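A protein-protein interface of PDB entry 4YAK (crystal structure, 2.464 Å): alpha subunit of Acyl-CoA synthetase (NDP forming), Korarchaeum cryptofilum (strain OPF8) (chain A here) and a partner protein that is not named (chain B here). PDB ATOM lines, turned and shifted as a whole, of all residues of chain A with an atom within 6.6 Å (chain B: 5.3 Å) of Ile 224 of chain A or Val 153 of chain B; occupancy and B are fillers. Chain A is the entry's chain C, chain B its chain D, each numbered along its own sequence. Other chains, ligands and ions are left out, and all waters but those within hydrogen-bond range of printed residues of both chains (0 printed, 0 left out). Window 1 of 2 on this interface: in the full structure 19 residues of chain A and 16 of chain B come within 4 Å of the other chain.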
ATOM      1  N   VAL A 193      -8.593  31.489 -18.074  1.00  0.00           N
ATOM      2  CA  VAL A 193      -7.678  31.881 -17.008  1.00  0.00           C
ATOM      3  C   VAL A 193      -6.631  32.870 -17.524  1.00  0.00           C
ATOM      4  O   VAL A 193      -6.320  33.865 -16.864  1.00  0.00           O
ATOM      5  CB  VAL A 193      -6.973  30.651 -16.407  1.00  0.00           C
ATOM      6  CG1 VAL A 193      -5.957  31.064 -15.340  1.00  0.00           C
ATOM      7  CG2 VAL A 193      -7.998  29.687 -15.825  1.00  0.00           C
ATOM      8  N   ARG A 219      -7.555  22.417 -14.322  1.00  0.00           N
ATOM      9  CA  ARG A 219      -7.446  23.852 -14.553  1.00  0.00           C
ATOM     10  C   ARG A 219      -8.354  24.642 -13.616  1.00  0.00           C
ATOM     11  O   ARG A 219      -8.203  25.849 -13.473  1.00  0.00           O
ATOM     12  CB  ARG A 219      -7.790  24.162 -16.007  1.00  0.00           C
ATOM     13  CG  ARG A 219      -7.517  25.582 -16.440  1.00  0.00           C
ATOM     14  CD  ARG A 219      -6.038  25.901 -16.379  1.00  0.00           C
ATOM     15  NE  ARG A 219      -5.725  27.163 -17.043  1.00  0.00           N
ATOM     16  CZ  ARG A 219      -4.513  27.700 -17.084  1.00  0.00           C
ATOM     17  NH1 ARG A 219      -3.496  27.090 -16.496  1.00  0.00           N
ATOM     18  NH2 ARG A 219      -4.318  28.849 -17.713  1.00  0.00           N
ATOM     19  N   GLY A 220      -9.289  23.955 -12.969  1.00  0.00           N
ATOM     20  CA  GLY A 220     -10.310  24.612 -12.168  1.00  0.00           C
ATOM     21  C   GLY A 220      -9.847  25.350 -10.930  1.00  0.00           C
ATOM     22  O   GLY A 220     -10.387  26.403 -10.598  1.00  0.00           O
ATOM     23  N   ARG A 221      -8.860  24.802 -10.235  1.00  0.00           N
ATOM     24  CA  ARG A 221      -8.337  25.444  -9.038  1.00  0.00           C
ATOM     25  C   ARG A 221      -7.738  26.807  -9.391  1.00  0.00           C
ATOM     26  O   ARG A 221      -7.998  27.809  -8.719  1.00  0.00           O
ATOM     27  CB  ARG A 221      -7.294  24.548  -8.366  1.00  0.00           C
ATOM     28  CG  ARG A 221      -6.762  25.069  -7.038  1.00  0.00           C
ATOM     29  CD  ARG A 221      -7.871  25.315  -6.003  1.00  0.00           C
ATOM     30  NE  ARG A 221      -8.201  26.736  -5.892  1.00  0.00           N
ATOM     31  CZ  ARG A 221      -8.953  27.271  -4.930  1.00  0.00           C
ATOM     32  NH1 ARG A 221      -9.184  28.578  -4.920  1.00  0.00           N
ATOM     33  NH2 ARG A 221      -9.464  26.515  -3.970  1.00  0.00           N
ATOM     34  N   MET A 222      -6.935  26.826 -10.449  1.00  0.00           N
ATOM     35  CA  MET A 222      -6.310  28.043 -10.923  1.00  0.00           C
ATOM     36  C   MET A 222      -7.383  29.027 -11.371  1.00  0.00           C
ATOM     37  O   MET A 222      -7.260  30.234 -11.166  1.00  0.00           O
ATOM     38  CB  MET A 222      -5.339  27.739 -12.073  1.00  0.00           C
ATOM     39  CG  MET A 222      -4.510  28.933 -12.578  1.00  0.00           C
ATOM     40  SD  MET A 222      -3.037  29.388 -11.610  1.00  0.00           S
ATOM     41  CE  MET A 222      -3.693  30.177 -10.134  1.00  0.00           C
ATOM     42  N   PHE A 223      -8.441  28.498 -11.977  1.00  0.00           N
ATOM     43  CA  PHE A 223      -9.556  29.318 -12.434  1.00  0.00           C
ATOM     44  C   PHE A 223     -10.184  30.078 -11.270  1.00  0.00           C
ATOM     45  O   PHE A 223     -10.564  31.242 -11.406  1.00  0.00           O
ATOM     46  CB  PHE A 223     -10.612  28.452 -13.131  1.00  0.00           C
ATOM     47  CG  PHE A 223     -11.811  29.228 -13.614  1.00  0.00           C
ATOM     48  CD1 PHE A 223     -11.826  29.787 -14.876  1.00  0.00           C
ATOM     49  CD2 PHE A 223     -12.917  29.403 -12.798  1.00  0.00           C
ATOM     50  CE1 PHE A 223     -12.922  30.509 -15.316  1.00  0.00           C
ATOM     51  CE2 PHE A 223     -14.012  30.124 -13.234  1.00  0.00           C
ATOM     52  CZ  PHE A 223     -14.014  30.674 -14.490  1.00  0.00           C
ATOM     53  N   ILE A 224     -10.296  29.421 -10.121  1.00  0.00           N
ATOM     54  CA  ILE A 224     -10.904  30.062  -8.968  1.00  0.00           C
ATOM     55  C   ILE A 224      -9.978  31.128  -8.408  1.00  0.00           C
ATOM     56  O   ILE A 224     -10.426  32.226  -8.096  1.00  0.00           O
ATOM     57  CB  ILE A 224     -11.253  29.049  -7.859  1.00  0.00           C
ATOM     58  CG1 ILE A 224     -12.301  28.056  -8.364  1.00  0.00           C
ATOM     59  CG2 ILE A 224     -11.784  29.775  -6.618  1.00  0.00           C
ATOM     60  CD1 ILE A 224     -12.570  26.910  -7.414  1.00  0.00           C
ATOM     61  N   ASP A 225      -8.696  30.800  -8.276  1.00  0.00           N
ATOM     62  CA  ASP A 225      -7.707  31.732  -7.739  1.00  0.00           C
ATOM     63  C   ASP A 225      -7.684  33.033  -8.530  1.00  0.00           C
ATOM     64  O   ASP A 225      -7.687  34.123  -7.953  1.00  0.00           O
ATOM     65  CB  ASP A 225      -6.309  31.102  -7.741  1.00  0.00           C
ATOM     66  CG  ASP A 225      -6.189  29.925  -6.778  1.00  0.00           C
ATOM     67  OD1 ASP A 225      -7.051  29.790  -5.881  1.00  0.00           O
ATOM     68  OD2 ASP A 225      -5.234  29.125  -6.921  1.00  0.00           O
ATOM     69  N   VAL A 226      -7.676  32.906  -9.853  1.00  0.00           N
ATOM     70  CA  VAL A 226      -7.624  34.058 -10.738  1.00  0.00           C
ATOM     71  C   VAL A 226      -8.949  34.808 -10.767  1.00  0.00           C
ATOM     72  O   VAL A 226      -8.977  36.021 -10.580  1.00  0.00           O
ATOM     73  CB  VAL A 226      -7.258  33.635 -12.172  1.00  0.00           C
ATOM     74  CG1 VAL A 226      -7.360  34.825 -13.152  1.00  0.00           C
ATOM     75  CG2 VAL A 226      -5.869  33.037 -12.188  1.00  0.00           C
ATOM     76  N   ALA A 227     -10.038  34.088 -11.012  1.00  0.00           N
ATOM     77  CA  ALA A 227     -11.343  34.722 -11.135  1.00  0.00           C
ATOM     78  C   ALA A 227     -11.690  35.434  -9.842  1.00  0.00           C
ATOM     79  O   ALA A 227     -12.170  36.570  -9.848  1.00  0.00           O
ATOM     80  CB  ALA A 227     -12.402  33.691 -11.483  1.00  0.00           C
ATOM     81  N   SER A 228     -11.371  34.782  -8.734  1.00  0.00           N
ATOM     82  CA  SER A 228     -11.690  35.306  -7.422  1.00  0.00           C
ATOM     83  C   SER A 228     -11.041  36.673  -7.174  1.00  0.00           C
ATOM     84  O   SER A 228     -11.694  37.585  -6.665  1.00  0.00           O
ATOM     85  CB  SER A 228     -11.248  34.302  -6.363  1.00  0.00           C
ATOM     86  OG  SER A 228     -11.469  34.808  -5.071  1.00  0.00           O
ATOM     87  N   ARG A 229      -9.775  36.823  -7.556  1.00  0.00           N
ATOM     88  CA  ARG A 229      -9.067  38.085  -7.354  1.00  0.00           C
ATOM     89  C   ARG A 229      -9.601  39.174  -8.288  1.00  0.00           C
ATOM     90  O   ARG A 229      -9.625  40.353  -7.933  1.00  0.00           O
ATOM     91  CB  ARG A 229      -7.562  37.910  -7.545  1.00  0.00           C
ATOM     92  CG  ARG A 229      -7.082  37.721  -8.983  1.00  0.00           C
ATOM     93  CD  ARG A 229      -5.713  38.363  -9.169  1.00  0.00           C
ATOM     94  NE  ARG A 229      -4.960  37.745 -10.257  1.00  0.00           N
ATOM     95  CZ  ARG A 229      -4.235  36.638 -10.132  1.00  0.00           C
ATOM     96  NH1 ARG A 229      -4.162  36.013  -8.957  1.00  0.00           N
ATOM     97  NH2 ARG A 229      -3.584  36.153 -11.186  1.00  0.00           N
ATOM     98  N   ILE A 264     -20.643  21.083  -8.848  1.00  0.00           N
ATOM     99  CA  ILE A 264     -19.318  21.545  -8.483  1.00  0.00           C
ATOM    100  C   ILE A 264     -18.938  22.824  -9.237  1.00  0.00           C
ATOM    101  O   ILE A 264     -18.258  23.691  -8.685  1.00  0.00           O
ATOM    102  CB  ILE A 264     -18.278  20.447  -8.732  1.00  0.00           C
ATOM    103  CG1 ILE A 264     -18.591  19.252  -7.828  1.00  0.00           C
ATOM    104  CG2 ILE A 264     -16.860  20.972  -8.473  1.00  0.00           C
ATOM    105  CD1 ILE A 264     -17.622  18.091  -7.954  1.00  0.00           C
ATOM    106  N   SER A 267     -20.533  25.654  -7.354  1.00  0.00           N
ATOM    107  CA  SER A 267     -19.764  25.971  -6.155  1.00  0.00           C
ATOM    108  C   SER A 267     -18.543  26.811  -6.508  1.00  0.00           C
ATOM    109  O   SER A 267     -18.254  27.800  -5.845  1.00  0.00           O
ATOM    110  CB  SER A 267     -19.325  24.694  -5.444  1.00  0.00           C
ATOM    111  OG  SER A 267     -20.440  24.006  -4.909  1.00  0.00           O
ATOM    112  N   ALA A 268     -17.810  26.389  -7.533  1.00  0.00           N
ATOM    113  CA  ALA A 268     -16.642  27.125  -8.007  1.00  0.00           C
ATOM    114  C   ALA A 268     -17.004  28.573  -8.363  1.00  0.00           C
ATOM    115  O   ALA A 268     -16.259  29.507  -8.073  1.00  0.00           O
ATOM    116  CB  ALA A 268     -16.033  26.421  -9.206  1.00  0.00           C
ATOM    117  N   PHE A 269     -18.162  28.764  -8.980  1.00  0.00           N
ATOM    118  CA  PHE A 269     -18.586  30.109  -9.339  1.00  0.00           C
ATOM    119  C   PHE A 269     -18.860  30.949  -8.097  1.00  0.00           C
ATOM    120  O   PHE A 269     -18.519  32.129  -8.066  1.00  0.00           O
ATOM    121  CB  PHE A 269     -19.820  30.050 -10.239  1.00  0.00           C
ATOM    122  CG  PHE A 269     -19.554  29.440 -11.585  1.00  0.00           C
ATOM    123  CD1 PHE A 269     -18.294  29.499 -12.158  1.00  0.00           C
ATOM    124  CD2 PHE A 269     -20.560  28.789 -12.270  1.00  0.00           C
ATOM    125  CE1 PHE A 269     -18.049  28.928 -13.396  1.00  0.00           C
ATOM    126  CE2 PHE A 269     -20.318  28.214 -13.505  1.00  0.00           C
ATOM    127  CZ  PHE A 269     -19.060  28.286 -14.066  1.00  0.00           C
ATOM    128  N   GLN A 271     -17.431  30.489  -5.131  1.00  0.00           N
ATOM    129  CA  GLN A 271     -16.128  30.751  -4.518  1.00  0.00           C
ATOM    130  C   GLN A 271     -15.313  31.788  -5.297  1.00  0.00           C
ATOM    131  O   GLN A 271     -14.365  32.360  -4.761  1.00  0.00           O
ATOM    132  CB  GLN A 271     -15.325  29.459  -4.390  1.00  0.00           C
ATOM    133  CG  GLN A 271     -16.000  28.397  -3.555  1.00  0.00           C
ATOM    134  CD  GLN A 271     -15.164  27.133  -3.424  1.00  0.00           C
ATOM    135  OE1 GLN A 271     -15.570  26.059  -3.863  1.00  0.00           O
ATOM    136  NE2 GLN A 271     -13.998  27.257  -2.810  1.00  0.00           N
ATOM    137  N   SER A 272     -15.680  32.028  -6.554  1.00  0.00           N
ATOM    138  CA  SER A 272     -14.972  32.988  -7.398  1.00  0.00           C
ATOM    139  C   SER A 272     -15.647  34.346  -7.405  1.00  0.00           C
ATOM    140  O   SER A 272     -15.118  35.279  -7.990  1.00  0.00           O
ATOM    141  CB  SER A 272     -14.873  32.482  -8.839  1.00  0.00           C
ATOM    142  OG  SER A 272     -14.208  31.234  -8.895  1.00  0.00           O
ATOM    143  N   PHE B 130     -11.610  20.596 -10.962  1.00  0.00           N
ATOM    144  CA  PHE B 130     -11.267  21.429  -9.813  1.00  0.00           C
ATOM    145  C   PHE B 130     -10.439  20.733  -8.745  1.00  0.00           C
ATOM    146  O   PHE B 130     -10.105  21.351  -7.734  1.00  0.00           O
ATOM    147  CB  PHE B 130     -12.549  21.985  -9.191  1.00  0.00           C
ATOM    148  CG  PHE B 130     -13.321  22.875 -10.123  1.00  0.00           C
ATOM    149  CD1 PHE B 130     -13.034  24.226 -10.215  1.00  0.00           C
ATOM    150  CD2 PHE B 130     -14.316  22.355 -10.927  1.00  0.00           C
ATOM    151  CE1 PHE B 130     -13.734  25.047 -11.086  1.00  0.00           C
ATOM    152  CE2 PHE B 130     -15.016  23.171 -11.794  1.00  0.00           C
ATOM    153  CZ  PHE B 130     -14.720  24.520 -11.871  1.00  0.00           C
ATOM    154  N   PRO B 132      -9.298  18.384  -5.600  1.00  0.00           N
ATOM    155  CA  PRO B 132      -9.935  17.982  -4.333  1.00  0.00           C
ATOM    156  C   PRO B 132     -11.118  18.869  -3.933  1.00  0.00           C
ATOM    157  O   PRO B 132     -10.995  20.093  -3.843  1.00  0.00           O
ATOM    158  CB  PRO B 132      -8.800  18.088  -3.309  1.00  0.00           C
ATOM    159  CG  PRO B 132      -7.783  18.972  -3.947  1.00  0.00           C
ATOM    160  CD  PRO B 132      -7.879  18.721  -5.413  1.00  0.00           C
ATOM    161  N   THR B 133     -12.258  18.227  -3.698  1.00  0.00           N
ATOM    162  CA  THR B 133     -13.497  18.914  -3.365  1.00  0.00           C
ATOM    163  C   THR B 133     -14.109  18.291  -2.116  1.00  0.00           C
ATOM    164  O   THR B 133     -14.204  17.073  -2.012  1.00  0.00           O
ATOM    165  CB  THR B 133     -14.529  18.830  -4.532  1.00  0.00           C
ATOM    166  OG1 THR B 133     -13.998  19.442  -5.715  1.00  0.00           O
ATOM    167  CG2 THR B 133     -15.847  19.508  -4.155  1.00  0.00           C
ATOM    168  N   VAL B 134     -14.536  19.134  -1.181  1.00  0.00           N
ATOM    169  CA  VAL B 134     -15.186  18.668   0.041  1.00  0.00           C
ATOM    170  C   VAL B 134     -16.706  18.684  -0.128  1.00  0.00           C
ATOM    171  O   VAL B 134     -17.269  19.632  -0.669  1.00  0.00           O
ATOM    172  CB  VAL B 134     -14.790  19.532   1.258  1.00  0.00           C
ATOM    173  CG1 VAL B 134     -15.592  19.155   2.494  1.00  0.00           C
ATOM    174  CG2 VAL B 134     -13.304  19.391   1.536  1.00  0.00           C
ATOM    175  N   PHE B 151     -21.126  21.383  -1.952  1.00  0.00           N
ATOM    176  CA  PHE B 151     -19.744  21.195  -2.370  1.00  0.00           C
ATOM    177  C   PHE B 151     -18.944  22.481  -2.271  1.00  0.00           C
ATOM    178  O   PHE B 151     -19.459  23.571  -2.544  1.00  0.00           O
ATOM    179  CB  PHE B 151     -19.688  20.692  -3.807  1.00  0.00           C
ATOM    180  CG  PHE B 151     -20.353  19.374  -4.016  1.00  0.00           C
ATOM    181  CD1 PHE B 151     -19.660  18.198  -3.811  1.00  0.00           C
ATOM    182  CD2 PHE B 151     -21.672  19.307  -4.439  1.00  0.00           C
ATOM    183  CE1 PHE B 151     -20.270  16.980  -4.016  1.00  0.00           C
ATOM    184  CE2 PHE B 151     -22.288  18.085  -4.645  1.00  0.00           C
ATOM    185  CZ  PHE B 151     -21.587  16.926  -4.435  1.00  0.00           C
ATOM    186  N   ARG B 152     -17.676  22.343  -1.892  1.00  0.00           N
ATOM    187  CA  ARG B 152     -16.716  23.440  -1.943  1.00  0.00           C
ATOM    188  C   ARG B 152     -15.372  22.896  -2.398  1.00  0.00           C
ATOM    189  O   ARG B 152     -14.965  21.814  -1.979  1.00  0.00           O
ATOM    190  CB  ARG B 152     -16.585  24.122  -0.581  1.00  0.00           C
ATOM    191  CG  ARG B 152     -17.774  24.971  -0.178  1.00  0.00           C
ATOM    192  CD  ARG B 152     -17.996  26.132  -1.150  1.00  0.00           C
ATOM    193  NE  ARG B 152     -18.962  27.091  -0.625  1.00  0.00           N
ATOM    194  CZ  ARG B 152     -20.277  26.902  -0.616  1.00  0.00           C
ATOM    195  NH1 ARG B 152     -20.793  25.788  -1.104  1.00  0.00           N
ATOM    196  NH2 ARG B 152     -21.080  27.828  -0.111  1.00  0.00           N
ATOM    197  N   VAL B 153     -14.694  23.638  -3.271  1.00  0.00           N
ATOM    198  CA  VAL B 153     -13.384  23.240  -3.773  1.00  0.00           C
ATOM    199  C   VAL B 153     -12.301  23.635  -2.767  1.00  0.00           C
ATOM    200  O   VAL B 153     -12.246  24.780  -2.328  1.00  0.00           O
ATOM    201  CB  VAL B 153     -13.087  23.894  -5.131  1.00  0.00           C
ATOM    202  CG1 VAL B 153     -11.749  23.420  -5.686  1.00  0.00           C
ATOM    203  CG2 VAL B 153     -14.204  23.602  -6.104  1.00  0.00           C
ATOM    204  N   ALA B 154     -11.455  22.677  -2.392  1.00  0.00           N
ATOM    205  CA  ALA B 154     -10.405  22.903  -1.403  1.00  0.00           C
ATOM    206  C   ALA B 154      -9.213  23.646  -2.014  1.00  0.00           C
ATOM    207  O   ALA B 154      -8.971  23.543  -3.221  1.00  0.00           O
ATOM    208  CB  ALA B 154      -9.955  21.571  -0.799  1.00  0.00           C
ATOM    209  N   PRO B 155      -8.450  24.385  -1.184  1.00  0.00           N
ATOM    210  CA  PRO B 155      -8.577  24.511   0.275  1.00  0.00           C
ATOM    211  C   PRO B 155      -9.740  25.385   0.703  1.00  0.00           C
ATOM    212  O   PRO B 155     -10.041  26.368   0.031  1.00  0.00           O
ATOM    213  CB  PRO B 155      -7.259  25.159   0.678  1.00  0.00           C
ATOM    214  CG  PRO B 155      -6.882  25.984  -0.497  1.00  0.00           C
ATOM    215  CD  PRO B 155      -7.337  25.208  -1.700  1.00  0.00           C
ATOM    216  N   LEU B 156     -10.366  25.032   1.821  1.00  0.00           N
ATOM    217  CA  LEU B 156     -11.534  25.740   2.327  1.00  0.00           C
ATOM    218  C   LEU B 156     -11.173  26.850   3.303  1.00  0.00           C
ATOM    219  O   LEU B 156     -10.437  26.631   4.271  1.00  0.00           O
ATOM    220  CB  LEU B 156     -12.492  24.763   3.015  1.00  0.00           C
ATOM    221  CG  LEU B 156     -13.619  24.168   2.171  1.00  0.00           C
ATOM    222  CD1 LEU B 156     -13.094  23.606   0.853  1.00  0.00           C
ATOM    223  CD2 LEU B 156     -14.337  23.084   2.965  1.00  0.00           C
ATOM    224  N   ASP B 160     -16.031  29.574   3.406  1.00  0.00           N
ATOM    225  CA  ASP B 160     -16.504  28.458   2.598  1.00  0.00           C
ATOM    226  C   ASP B 160     -17.190  27.424   3.485  1.00  0.00           C
ATOM    227  O   ASP B 160     -18.288  26.961   3.184  1.00  0.00           O
ATOM    228  CB  ASP B 160     -15.344  27.798   1.840  1.00  0.00           C
ATOM    229  CG  ASP B 160     -14.777  28.676   0.742  1.00  0.00           C
ATOM    230  OD1 ASP B 160     -15.560  29.411   0.107  1.00  0.00           O
ATOM    231  OD2 ASP B 160     -13.550  28.619   0.504  1.00  0.00           O
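O of Ala 154 of chain B is in hydrogen-bond range of NH2 of Arg 221 of chain A, at 3.1 Å. O of Phe 151 of chain B sits at hydrogen-bond distance from OG of Ser 267 of chain A (2.6 Å). The side-chain amide oxygen (OE1) of Gln 271 of chain A lies within hydrogen-bond range of the backbone NH (N) of Val 153 of chain B.
NH1 of Arg 221 of chain A lies within salt-bridge range of OD1 of Asp 225 of chain A (2.6 Å). The backbone carbonyl oxygen (O) of Ala 268 of chain A is in hydrogen-bond range of the side-chain hydroxyl (OG) of Ser 272 of chain A, at 2.8 Å. The backbone carbonyl oxygen (O) of Pro 132 of chain B is in hydrogen-bond range of the backbone NH (N) of Ala 154 of chain B (3.0 Å). The backbone carbonyl oxygen of Arg 152 of chain B lies within hydrogen-bond range of the backbone NH of Val 134 of chain B (2.8 Å).
Phe 130 of chain B touches Gly 220 of chain A (CD1 to CA, 3.4 Å). O of Val 153 of chain B touches NH2 of Arg 221 of chain A (3.7 Å). NH2 of Arg 221 of chain A touches CD of Pro 155 of chain B, 3.4 Å away. Phe 130 of chain B touches Ile 224 of chain A. Ile 224 of chain A touches Val 153 of chain B (CD1 to CB, 3.8 Å). CD2 of Phe 130 of chain B touches CG2 of Ile 264 of chain A (3.8 Å). Ala 268 of chain A touches Phe 130 of chain B (CB to CE1, 3.3 Å). Gln 271 of chain A touches Arg 152 of chain B. Gln 271 of chain A touches Asp 160 of chain B (NE2 to OD2, 3.6 Å).
Of chain B, only Phe 130 and Val 153 come within 4 Å of Ile 224 of chain A. Of chain A, only Arg 221, Ile 224 and Gln 271 come within 4 Å of Val 153 of chain B. Of the printed residues of chain B, Ala 268 of chain A touches Phe 130 (3.3 Å). Of the printed residues of chain B, Arg 221 of chain A touches Val 153 (3.7 Å), Ala 154 (3.1 Å) and Pro 155 (3.4 Å). Of the printed residues of chain A, Asp 160 of chain B touches Gln 271. The nearest printed residue of chain B that does not touch Ile 224 of chain A is Ala 154 of chain B (6.5 Å). The nearest printed residue of chain B that does not touch Ser 267 of chain A is Arg 152 of chain B (4.2 Å).
Along chain B the printed residues that touch a printed residue of chain A span positions 130 to 160. Printed residues of chain A that touch a printed residue of chain B: Gly 220, Arg 221, Ile 224, Ile 264, Ser 267, Ala 268 and Gln 271. Among the printed residues, 12 pairs touch across the chains.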
